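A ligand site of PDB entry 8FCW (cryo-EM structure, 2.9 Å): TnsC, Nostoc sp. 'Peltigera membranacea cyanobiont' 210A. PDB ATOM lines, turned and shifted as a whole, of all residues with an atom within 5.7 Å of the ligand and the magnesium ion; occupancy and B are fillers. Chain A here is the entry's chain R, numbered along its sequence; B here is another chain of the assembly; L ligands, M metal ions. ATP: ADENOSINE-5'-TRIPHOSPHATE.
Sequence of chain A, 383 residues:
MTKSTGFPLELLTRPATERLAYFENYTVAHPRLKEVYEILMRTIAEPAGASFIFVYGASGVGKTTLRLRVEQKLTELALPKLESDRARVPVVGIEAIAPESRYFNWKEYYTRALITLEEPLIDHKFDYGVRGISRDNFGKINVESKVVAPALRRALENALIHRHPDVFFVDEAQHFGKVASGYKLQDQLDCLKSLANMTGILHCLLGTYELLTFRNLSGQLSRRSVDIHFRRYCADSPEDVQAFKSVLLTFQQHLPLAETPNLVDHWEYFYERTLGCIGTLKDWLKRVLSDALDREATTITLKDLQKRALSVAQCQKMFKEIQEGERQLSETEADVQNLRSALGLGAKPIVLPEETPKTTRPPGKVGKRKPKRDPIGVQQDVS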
ATOM      1  N   GLU A  24      16.823 -30.819   2.568  1.00  0.00           N
ATOM      2  CA  GLU A  24      16.535 -29.416   2.900  1.00  0.00           C
ATOM      3  C   GLU A  24      17.798 -28.580   2.922  1.00  0.00           C
ATOM      4  O   GLU A  24      17.777 -27.401   2.544  1.00  0.00           O
ATOM      5  CB  GLU A  24      15.779 -29.308   4.241  1.00  0.00           C
ATOM      6  CG  GLU A  24      16.512 -29.814   5.470  1.00  0.00           C
ATOM      7  CD  GLU A  24      17.471 -28.800   6.056  1.00  0.00           C
ATOM      8  OE1 GLU A  24      17.417 -27.621   5.658  1.00  0.00           O
ATOM      9  OE2 GLU A  24      18.279 -29.175   6.929  1.00  0.00           O
ATOM     10  N   TYR A  26      20.452 -29.107   1.107  1.00  0.00           N
ATOM     11  CA  TYR A  26      21.054 -29.051  -0.217  1.00  0.00           C
ATOM     12  C   TYR A  26      20.565 -27.822  -0.956  1.00  0.00           C
ATOM     13  O   TYR A  26      19.383 -27.542  -0.976  1.00  0.00           O
ATOM     14  CB  TYR A  26      20.738 -30.324  -1.007  1.00  0.00           C
ATOM     15  CG  TYR A  26      20.980 -30.217  -2.487  1.00  0.00           C
ATOM     16  CD1 TYR A  26      19.976 -29.807  -3.335  1.00  0.00           C
ATOM     17  CD2 TYR A  26      22.200 -30.575  -3.043  1.00  0.00           C
ATOM     18  CE1 TYR A  26      20.177 -29.714  -4.701  1.00  0.00           C
ATOM     19  CE2 TYR A  26      22.413 -30.487  -4.414  1.00  0.00           C
ATOM     20  CZ  TYR A  26      21.389 -30.057  -5.232  1.00  0.00           C
ATOM     21  OH  TYR A  26      21.601 -29.973  -6.581  1.00  0.00           O
ATOM     22  N   THR A  27      21.499 -27.100  -1.555  1.00  0.00           N
ATOM     23  CA  THR A  27      21.198 -25.897  -2.327  1.00  0.00           C
ATOM     24  C   THR A  27      21.684 -26.081  -3.753  1.00  0.00           C
ATOM     25  O   THR A  27      22.826 -26.459  -3.975  1.00  0.00           O
ATOM     26  CB  THR A  27      21.854 -24.664  -1.707  1.00  0.00           C
ATOM     27  OG1 THR A  27      23.226 -24.954  -1.408  1.00  0.00           O
ATOM     28  CG2 THR A  27      21.145 -24.265  -0.430  1.00  0.00           C
ATOM     29  N   VAL A  28      20.797 -25.826  -4.701  1.00  0.00           N
ATOM     30  CA  VAL A  28      21.114 -25.940  -6.112  1.00  0.00           C
ATOM     31  C   VAL A  28      21.497 -24.580  -6.645  1.00  0.00           C
ATOM     32  O   VAL A  28      21.070 -23.548  -6.134  1.00  0.00           O
ATOM     33  CB  VAL A  28      19.934 -26.520  -6.903  1.00  0.00           C
ATOM     34  CG1 VAL A  28      18.816 -25.489  -7.073  1.00  0.00           C
ATOM     35  CG2 VAL A  28      20.383 -27.058  -8.257  1.00  0.00           C
ATOM     36  N   ALA A  29      22.353 -24.576  -7.671  1.00  0.00           N
ATOM     37  CA  ALA A  29      22.796 -23.351  -8.302  1.00  0.00           C
ATOM     38  C   ALA A  29      22.212 -23.272  -9.695  1.00  0.00           C
ATOM     39  O   ALA A  29      22.314 -24.208 -10.485  1.00  0.00           O
ATOM     40  CB  ALA A  29      24.313 -23.307  -8.356  1.00  0.00           C
ATOM     41  N   HIS A  30      21.602 -22.121  -9.986  1.00  0.00           N
ATOM     42  CA  HIS A  30      20.971 -21.871 -11.264  1.00  0.00           C
ATOM     43  C   HIS A  30      21.428 -20.537 -11.794  1.00  0.00           C
ATOM     44  O   HIS A  30      21.843 -19.658 -11.019  1.00  0.00           O
ATOM     45  CB  HIS A  30      19.447 -21.923 -11.121  1.00  0.00           C
ATOM     46  CG  HIS A  30      18.902 -21.187  -9.946  1.00  0.00           C
ATOM     47  ND1 HIS A  30      18.101 -20.066 -10.072  1.00  0.00           N
ATOM     48  CD2 HIS A  30      19.012 -21.420  -8.619  1.00  0.00           C
ATOM     49  CE1 HIS A  30      17.755 -19.647  -8.867  1.00  0.00           C
ATOM     50  NE2 HIS A  30      18.291 -20.444  -7.967  1.00  0.00           N
ATOM     51  N   LEU A  33      20.384 -17.159 -10.102  1.00  0.00           N
ATOM     52  CA  LEU A  33      20.930 -17.006  -8.760  1.00  0.00           C
ATOM     53  C   LEU A  33      22.401 -16.641  -8.808  1.00  0.00           C
ATOM     54  O   LEU A  33      22.864 -15.756  -8.085  1.00  0.00           O
ATOM     55  CB  LEU A  33      20.723 -18.281  -7.954  1.00  0.00           C
ATOM     56  CG  LEU A  33      21.418 -18.366  -6.584  1.00  0.00           C
ATOM     57  CD1 LEU A  33      21.001 -17.217  -5.680  1.00  0.00           C
ATOM     58  CD2 LEU A  33      21.113 -19.699  -5.943  1.00  0.00           C
ATOM     59  N   ALA A  58      10.161 -11.907  -6.584  1.00  0.00           N
ATOM     60  CA  ALA A  58       8.892 -12.486  -6.174  1.00  0.00           C
ATOM     61  C   ALA A  58       9.079 -13.341  -4.926  1.00  0.00           C
ATOM     62  O   ALA A  58      10.192 -13.686  -4.544  1.00  0.00           O
ATOM     63  CB  ALA A  58       8.276 -13.294  -7.299  1.00  0.00           C
ATOM     64  N   SER A  59       7.954 -13.756  -4.349  1.00  0.00           N
ATOM     65  CA  SER A  59       8.041 -14.655  -3.223  1.00  0.00           C
ATOM     66  C   SER A  59       8.369 -16.042  -3.755  1.00  0.00           C
ATOM     67  O   SER A  59       7.485 -16.778  -4.179  1.00  0.00           O
ATOM     68  CB  SER A  59       6.719 -14.690  -2.450  1.00  0.00           C
ATOM     69  OG  SER A  59       6.927 -15.146  -1.117  1.00  0.00           O
ATOM     70  N   GLY A  60       9.661 -16.390  -3.779  1.00  0.00           N
ATOM     71  CA  GLY A  60      10.071 -17.703  -4.227  1.00  0.00           C
ATOM     72  C   GLY A  60      11.353 -17.666  -5.038  1.00  0.00           C
ATOM     73  O   GLY A  60      11.873 -18.713  -5.424  1.00  0.00           O
ATOM     74  N   VAL A  61      11.867 -16.462  -5.288  1.00  0.00           N
ATOM     75  CA  VAL A  61      13.067 -16.328  -6.098  1.00  0.00           C
ATOM     76  C   VAL A  61      14.331 -16.756  -5.356  1.00  0.00           C
ATOM     77  O   VAL A  61      15.335 -17.093  -5.986  1.00  0.00           O
ATOM     78  CB  VAL A  61      13.241 -14.875  -6.601  1.00  0.00           C
ATOM     79  CG1 VAL A  61      12.062 -14.480  -7.464  1.00  0.00           C
ATOM     80  CG2 VAL A  61      13.391 -13.930  -5.417  1.00  0.00           C
ATOM     81  N   GLY A  62      14.293 -16.731  -4.034  1.00  0.00           N
ATOM     82  CA  GLY A  62      15.455 -17.109  -3.251  1.00  0.00           C
ATOM     83  C   GLY A  62      16.185 -15.912  -2.693  1.00  0.00           C
ATOM     84  O   GLY A  62      17.416 -15.889  -2.662  1.00  0.00           O
ATOM     85  N   LYS A  63      15.441 -14.900  -2.259  1.00  0.00           N
ATOM     86  CA  LYS A  63      16.044 -13.711  -1.703  1.00  0.00           C
ATOM     87  C   LYS A  63      16.725 -14.002  -0.379  1.00  0.00           C
ATOM     88  O   LYS A  63      17.861 -13.591  -0.152  1.00  0.00           O
ATOM     89  CB  LYS A  63      15.011 -12.609  -1.552  1.00  0.00           C
ATOM     90  CG  LYS A  63      14.539 -12.004  -2.865  1.00  0.00           C
ATOM     91  CD  LYS A  63      13.501 -10.930  -2.614  1.00  0.00           C
ATOM     92  CE  LYS A  63      12.237 -11.509  -1.990  1.00  0.00           C
ATOM     93  NZ  LYS A  63      11.547 -12.457  -2.912  1.00  0.00           N
ATOM     94  N   THR A  64      16.043 -14.701   0.517  1.00  0.00           N
ATOM     95  CA  THR A  64      16.586 -14.951   1.842  1.00  0.00           C
ATOM     96  C   THR A  64      17.807 -15.857   1.775  1.00  0.00           C
ATOM     97  O   THR A  64      18.797 -15.625   2.473  1.00  0.00           O
ATOM     98  CB  THR A  64      15.530 -15.557   2.770  1.00  0.00           C
ATOM     99  OG1 THR A  64      14.260 -14.976   2.482  1.00  0.00           O
ATOM    100  CG2 THR A  64      15.877 -15.273   4.214  1.00  0.00           C
ATOM    101  N   THR A  65      17.765 -16.878   0.937  1.00  0.00           N
ATOM    102  CA  THR A  65      18.911 -17.764   0.824  1.00  0.00           C
ATOM    103  C   THR A  65      20.111 -17.067   0.182  1.00  0.00           C
ATOM    104  O   THR A  65      21.257 -17.310   0.562  1.00  0.00           O
ATOM    105  CB  THR A  65      18.558 -19.045   0.050  1.00  0.00           C
ATOM    106  OG1 THR A  65      19.741 -19.823  -0.165  1.00  0.00           O
ATOM    107  CG2 THR A  65      17.945 -18.702  -1.280  1.00  0.00           C
ATOM    108  N   LEU A  66      19.854 -16.180  -0.767  1.00  0.00           N
ATOM    109  CA  LEU A  66      20.928 -15.382  -1.337  1.00  0.00           C
ATOM    110  C   LEU A  66      21.537 -14.451  -0.318  1.00  0.00           C
ATOM    111  O   LEU A  66      22.756 -14.284  -0.263  1.00  0.00           O
ATOM    112  CB  LEU A  66      20.423 -14.598  -2.552  1.00  0.00           C
ATOM    113  CG  LEU A  66      21.345 -13.567  -3.193  1.00  0.00           C
ATOM    114  CD1 LEU A  66      21.176 -13.650  -4.688  1.00  0.00           C
ATOM    115  CD2 LEU A  66      20.973 -12.183  -2.685  1.00  0.00           C
ATOM    116  N   GLU A 172      12.462  -8.330   3.818  1.00  0.00           N
ATOM    117  CA  GLU A 172      11.114  -7.848   3.540  1.00  0.00           C
ATOM    118  C   GLU A 172      10.996  -6.351   3.792  1.00  0.00           C
ATOM    119  O   GLU A 172      10.191  -5.905   4.601  1.00  0.00           O
ATOM    120  CB  GLU A 172      10.060  -8.650   4.329  1.00  0.00           C
ATOM    121  CG  GLU A 172      10.191  -8.696   5.841  1.00  0.00           C
ATOM    122  CD  GLU A 172      11.201  -9.719   6.303  1.00  0.00           C
ATOM    123  OE1 GLU A 172      11.559 -10.603   5.507  1.00  0.00           O
ATOM    124  OE2 GLU A 172      11.649  -9.620   7.459  1.00  0.00           O
ATOM    125  N   GLY A 207      13.077  -7.407  -0.710  1.00  0.00           N
ATOM    126  CA  GLY A 207      11.659  -7.510  -0.513  1.00  0.00           C
ATOM    127  C   GLY A 207      10.954  -7.986  -1.756  1.00  0.00           C
ATOM    128  O   GLY A 207      11.559  -8.286  -2.765  1.00  0.00           O
ATOM    129  N   THR A 208       9.631  -8.056  -1.662  1.00  0.00           N
ATOM    130  CA  THR A 208       8.810  -8.528  -2.750  1.00  0.00           C
ATOM    131  C   THR A 208       8.638  -7.417  -3.779  1.00  0.00           C
ATOM    132  O   THR A 208       9.273  -6.371  -3.688  1.00  0.00           O
ATOM    133  CB  THR A 208       7.451  -9.020  -2.228  1.00  0.00           C
ATOM    134  OG1 THR A 208       6.598  -7.914  -1.978  1.00  0.00           O
ATOM    135  CG2 THR A 208       7.637  -9.847  -0.949  1.00  0.00           C
ATOM    136  N   PHE A 251      17.225 -31.662  -9.176  1.00  0.00           N
ATOM    137  CA  PHE A 251      16.438 -31.960  -7.981  1.00  0.00           C
ATOM    138  C   PHE A 251      16.004 -33.420  -7.978  1.00  0.00           C
ATOM    139  O   PHE A 251      16.039 -34.064  -6.941  1.00  0.00           O
ATOM    140  CB  PHE A 251      15.225 -31.041  -7.907  1.00  0.00           C
ATOM    141  CG  PHE A 251      15.425 -29.828  -7.037  1.00  0.00           C
ATOM    142  CD1 PHE A 251      16.203 -29.904  -5.917  1.00  0.00           C
ATOM    143  CD2 PHE A 251      14.826 -28.625  -7.354  1.00  0.00           C
ATOM    144  CE1 PHE A 251      16.385 -28.800  -5.103  1.00  0.00           C
ATOM    145  CE2 PHE A 251      15.012 -27.517  -6.553  1.00  0.00           C
ATOM    146  CZ  PHE A 251      15.803 -27.598  -5.438  1.00  0.00           C
ATOM    147  N   ILE A 278      12.364 -20.969  -7.763  1.00  0.00           N
ATOM    148  CA  ILE A 278      13.120 -22.117  -7.316  1.00  0.00           C
ATOM    149  C   ILE A 278      12.784 -22.454  -5.872  1.00  0.00           C
ATOM    150  O   ILE A 278      12.712 -23.615  -5.500  1.00  0.00           O
ATOM    151  CB  ILE A 278      14.632 -21.860  -7.478  1.00  0.00           C
ATOM    152  CG1 ILE A 278      14.985 -21.740  -8.959  1.00  0.00           C
ATOM    153  CG2 ILE A 278      15.448 -22.961  -6.829  1.00  0.00           C
ATOM    154  CD1 ILE A 278      14.318 -22.781  -9.847  1.00  0.00           C
ATOM    155  N   GLY A 279      12.557 -21.445  -5.043  1.00  0.00           N
ATOM    156  CA  GLY A 279      12.215 -21.675  -3.663  1.00  0.00           C
ATOM    157  C   GLY A 279      10.881 -22.383  -3.505  1.00  0.00           C
ATOM    158  O   GLY A 279      10.742 -23.303  -2.698  1.00  0.00           O
ATOM    159  N   THR A 280       9.892 -21.959  -4.273  1.00  0.00           N
ATOM    160  CA  THR A 280       8.589 -22.594  -4.215  1.00  0.00           C
ATOM    161  C   THR A 280       8.662 -24.045  -4.666  1.00  0.00           C
ATOM    162  O   THR A 280       8.046 -24.919  -4.075  1.00  0.00           O
ATOM    163  CB  THR A 280       7.584 -21.813  -5.066  1.00  0.00           C
ATOM    164  OG1 THR A 280       7.664 -20.420  -4.742  1.00  0.00           O
ATOM    165  CG2 THR A 280       6.181 -22.282  -4.796  1.00  0.00           C
ATOM    166  N   LYS A 282      11.300 -25.916  -4.479  1.00  0.00           N
ATOM    167  CA  LYS A 282      12.007 -26.622  -3.433  1.00  0.00           C
ATOM    168  C   LYS A 282      11.076 -26.982  -2.287  1.00  0.00           C
ATOM    169  O   LYS A 282      11.136 -28.091  -1.763  1.00  0.00           O
ATOM    170  CB  LYS A 282      13.178 -25.793  -2.921  1.00  0.00           C
ATOM    171  CG  LYS A 282      13.831 -26.317  -1.649  1.00  0.00           C
ATOM    172  CD  LYS A 282      14.456 -27.673  -1.881  1.00  0.00           C
ATOM    173  CE  LYS A 282      15.262 -28.102  -0.672  1.00  0.00           C
ATOM    174  NZ  LYS A 282      16.311 -27.107  -0.350  1.00  0.00           N
ATOM    175  N   ASP A 283      10.211 -26.056  -1.901  1.00  0.00           N
ATOM    176  CA  ASP A 283       9.285 -26.351  -0.811  1.00  0.00           C
ATOM    177  C   ASP A 283       8.289 -27.417  -1.231  1.00  0.00           C
ATOM    178  O   ASP A 283       7.948 -28.298  -0.438  1.00  0.00           O
ATOM    179  CB  ASP A 283       8.551 -25.084  -0.373  1.00  0.00           C
ATOM    180  CG  ASP A 283       9.503 -23.955  -0.044  1.00  0.00           C
ATOM    181  OD1 ASP A 283      10.532 -24.213   0.609  1.00  0.00           O
ATOM    182  OD2 ASP A 283       9.207 -22.801  -0.429  1.00  0.00           O
ATOM    183  N   ALA B  48       7.591 -26.620   5.455  1.00  0.00           N
ATOM    184  CA  ALA B  48       8.313 -26.352   4.211  1.00  0.00           C
ATOM    185  C   ALA B  48       8.109 -24.927   3.732  1.00  0.00           C
ATOM    186  O   ALA B  48       7.544 -24.674   2.675  1.00  0.00           O
ATOM    187  CB  ALA B  48       7.916 -27.351   3.138  1.00  0.00           C
ATOM    188  N   GLY B  49       8.536 -23.998   4.566  1.00  0.00           N
ATOM    189  CA  GLY B  49       8.473 -22.593   4.236  1.00  0.00           C
ATOM    190  C   GLY B  49       7.070 -22.049   4.185  1.00  0.00           C
ATOM    191  O   GLY B  49       6.746 -21.197   3.350  1.00  0.00           O
ATOM    192  N   GLN B 220       2.846 -12.697  -1.468  1.00  0.00           N
ATOM    193  CA  GLN B 220       3.798 -13.132  -0.459  1.00  0.00           C
ATOM    194  C   GLN B 220       3.109 -13.920   0.635  1.00  0.00           C
ATOM    195  O   GLN B 220       3.612 -14.945   1.098  1.00  0.00           O
ATOM    196  CB  GLN B 220       4.535 -11.926   0.129  1.00  0.00           C
ATOM    197  CG  GLN B 220       5.217 -12.172   1.451  1.00  0.00           C
ATOM    198  CD  GLN B 220       6.518 -12.923   1.297  1.00  0.00           C
ATOM    199  OE1 GLN B 220       7.150 -12.897   0.243  1.00  0.00           O
ATOM    200  NE2 GLN B 220       6.935 -13.599   2.363  1.00  0.00           N
ATOM    201  N   ARG B 223       2.006 -17.363  -0.661  1.00  0.00           N
ATOM    202  CA  ARG B 223       3.012 -18.405  -0.780  1.00  0.00           C
ATOM    203  C   ARG B 223       3.126 -19.198   0.507  1.00  0.00           C
ATOM    204  O   ARG B 223       3.312 -20.415   0.462  1.00  0.00           O
ATOM    205  CB  ARG B 223       4.376 -17.828  -1.132  1.00  0.00           C
ATOM    206  CG  ARG B 223       5.426 -18.881  -1.474  1.00  0.00           C
ATOM    207  CD  ARG B 223       6.808 -18.278  -1.607  1.00  0.00           C
ATOM    208  NE  ARG B 223       7.782 -18.978  -0.798  1.00  0.00           N
ATOM    209  CZ  ARG B 223       8.299 -18.507   0.327  1.00  0.00           C
ATOM    210  NH1 ARG B 223       7.957 -17.313   0.802  1.00  0.00           N
ATOM    211  NH2 ARG B 223       9.140 -19.254   1.017  1.00  0.00           N
ATOM    212  N   ARG B 224       3.042 -18.518   1.647  1.00  0.00           N
ATOM    213  CA  ARG B 224       3.313 -19.169   2.934  1.00  0.00           C
ATOM    214  C   ARG B 224       2.048 -19.548   3.676  1.00  0.00           C
ATOM    215  O   ARG B 224       2.035 -19.576   4.911  1.00  0.00           O
ATOM    216  CB  ARG B 224       4.179 -18.261   3.806  1.00  0.00           C
ATOM    217  CG  ARG B 224       5.000 -17.289   2.992  1.00  0.00           C
ATOM    218  CD  ARG B 224       5.841 -16.393   3.874  1.00  0.00           C
ATOM    219  NE  ARG B 224       7.121 -17.010   4.202  1.00  0.00           N
ATOM    220  CZ  ARG B 224       8.196 -16.354   4.592  1.00  0.00           C
ATOM    221  NH1 ARG B 224       8.179 -15.025   4.719  1.00  0.00           N
ATOM    222  NH2 ARG B 224       9.309 -17.011   4.870  1.00  0.00           N
HETATM  223  PG  ATP L   1      10.629 -14.137   1.260  1.00  0.00           P
HETATM  224  O1G ATP L   1       9.595 -15.212   1.546  1.00  0.00           O
HETATM  225  O2G ATP L   1      10.060 -12.776   0.854  1.00  0.00           O
HETATM  226  O3G ATP L   1      11.583 -13.992   2.405  1.00  0.00           O
HETATM  227  PB  ATP L   1      11.505 -15.646  -1.198  1.00  0.00           P
HETATM  228  O1B ATP L   1      12.454 -15.290  -2.276  1.00  0.00           O
HETATM  229  O2B ATP L   1      10.095 -15.681  -1.479  1.00  0.00           O
HETATM  230  O3B ATP L   1      11.558 -14.577  -0.019  1.00  0.00           O
HETATM  231  PA  ATP L   1      13.276 -17.842  -0.334  1.00  0.00           P
HETATM  232  O1A ATP L   1      13.360 -18.808  -1.462  1.00  0.00           O
HETATM  233  O2A ATP L   1      14.419 -16.894  -0.157  1.00  0.00           O
HETATM  234  O3A ATP L   1      11.925 -16.989  -0.473  1.00  0.00           O
HETATM  235  O5' ATP L   1      13.056 -18.624   1.045  1.00  0.00           O
HETATM  236  C5' ATP L   1      13.978 -19.613   1.477  1.00  0.00           C
HETATM  237  C4' ATP L   1      13.418 -21.003   1.197  1.00  0.00           C
HETATM  238  O4' ATP L   1      13.587 -21.303  -0.186  1.00  0.00           O
HETATM  239  C3' ATP L   1      14.136 -22.097   1.961  1.00  0.00           C
HETATM  240  O3' ATP L   1      13.224 -23.159   2.273  1.00  0.00           O
HETATM  241  C2' ATP L   1      15.200 -22.553   0.994  1.00  0.00           C
HETATM  242  O2' ATP L   1      15.592 -23.902   1.212  1.00  0.00           O
HETATM  243  C1' ATP L   1      14.498 -22.400  -0.342  1.00  0.00           C
HETATM  244  N9  ATP L   1      15.414 -22.092  -1.470  1.00  0.00           N
HETATM  245  C8  ATP L   1      15.387 -20.986  -2.234  1.00  0.00           C
HETATM  246  N7  ATP L   1      16.313 -20.997  -3.191  1.00  0.00           N
HETATM  247  C5  ATP L   1      16.948 -22.170  -3.040  1.00  0.00           C
HETATM  248  C6  ATP L   1      18.025 -22.833  -3.698  1.00  0.00           C
HETATM  249  N6  ATP L   1      18.645 -22.270  -4.730  1.00  0.00           N
HETATM  250  N1  ATP L   1      18.403 -24.038  -3.259  1.00  0.00           N
HETATM  251  C2  ATP L   1      17.783 -24.601  -2.227  1.00  0.00           C
HETATM  252  N3  ATP L   1      16.788 -24.088  -1.515  1.00  0.00           N
HETATM  253  C4  ATP L   1      16.352 -22.889  -1.930  1.00  0.00           C
HETATM  254 MG    MG M   1      12.709 -15.873   1.078  1.00  0.00          MG
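The guanidinium group (NH1) of Arg 223 of chain B lies within hydrogen-bond range of the side-chain hydroxyl (OG) of Ser 59, 3.1 Å away.
The side-chain amino group of Lys 63 sits at hydrogen-bond distance from the backbone carbonyl oxygen of Ala 58 (2.5 Å).
O of Tyr 26 is in hydrogen-bond range of NZ of Lys 282.
The side-chain amide oxygen (OE1) of Gln 220 of chain B sits at hydrogen-bond distance from the side-chain hydroxyl (OG) of Ser 59.
NE2 of Gln 220 of chain B sits close to NH1 of Arg 224 of chain B (3.0 Å).
O of Gly 60 is in hydrogen-bond range of N of Gly 279 (2.8 Å).
The side-chain amino group (NZ) of Lys 282 lies within hydrogen-bond range of the backbone carbonyl oxygen (O) of Glu 24 (3.3 Å).
The backbone carbonyl oxygen (O) of Gly 60 lies within hydrogen-bond range of the backbone NH (N) of Ile 278 (3.3 Å).
NZ of Lys 63 is in salt-bridge range of O1B of the ligand (3.0 Å).
The guanidinium group of Arg 224 of chain B is in salt-bridge range of an oxygen (O1G) of the ligand, at 3.5 Å.
O1G of the ligand is in salt-bridge range of NH1 of Arg 223 of chain B (2.8 Å).
The backbone NH of Thr 64 lies close to an oxygen (O2A) of the ligand, at 2.8 Å.
An oxygen (O2B) of the ligand sits at hydrogen-bond distance from the backbone NH of Gly 60, 2.4 Å away.
The backbone carbonyl oxygen of Val 28 lies within hydrogen-bond range of a nitrogen (N6) of the ligand (3.1 Å).
O2B of the ligand sits close to OG of Ser 59 (3.2 Å).
The backbone NH (N) of Lys 63 is in hydrogen-bond range of an oxygen (O1B) of the ligand (3.0 Å).
The backbone NH of Val 61 sits at hydrogen-bond distance from an oxygen (O1B) of the ligand.
The side-chain carboxylate (OD1) of Asp 283 is in hydrogen-bond range of an oxygen (O3') of the ligand, at 3.3 Å.
The backbone NH (N) of Val 28 is in hydrogen-bond range of a nitrogen (N1) of the ligand, at 3.3 Å.
An oxygen (O1B) of the ligand is in hydrogen-bond range of the backbone NH of Gly 62, at 2.9 Å.
The side-chain amide oxygen (OE1) of Gln 220 of chain B lies close to an oxygen (O2G) of the ligand, at 3.0 Å.
The side-chain amino group (NZ) of Lys 282 lies within hydrogen-bond range of a nitrogen (N3) of the ligand (3.3 Å).
The magnesium ion is bound by an oxygen (O3B) of the ligand (2.1 Å), an oxygen (O3A) of the ligand (2.1 Å), the side-chain hydroxyl (OG1) of Thr 64 (2.3 Å), an oxygen (O2A) of the ligand (2.3 Å) and an oxygen (O3G) of the ligand (2.6 Å).
The magnesium ion has five donor atoms within binding distance.
Slightly farther from the magnesium ion lies O5' of the ligand (2.8 Å).
O of Tyr 26 touches C2 of the ligand, at 3.6 Å.
Thr 27 touches the ligand (CA to N1, 3.5 Å).
His 30 touches the ligand.
CD2 of Leu 33 touches N6 of the ligand (3.8 Å).
O of Ala 58 touches O1B of the ligand, 3.6 Å away.
CG2 of Thr 65 touches N7 of the ligand, at 3.4 Å.
Ile 278 touches the ligand.
Gly 279 touches the ligand (CA to C8, 3.5 Å).
Hydrophobic or aromatic side chains that line the ligand: Val 28, His 30, Leu 33, Val 61 and Ile 278.
20 residues have an atom within 4 Å of the ligand: Tyr 26, Thr 27, Val 28, His 30, Leu 33, Ala 58, Ser 59, Gly 60, Val 61, Gly 62, Lys 63, Thr 64, Thr 65, Ile 278, Gly 279, Lys 282, Asp 283, Gln 220 of chain B, Arg 223 of chain B and Arg 224 of chain B.
Within 4 Å of the magnesium ion: Thr 64.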
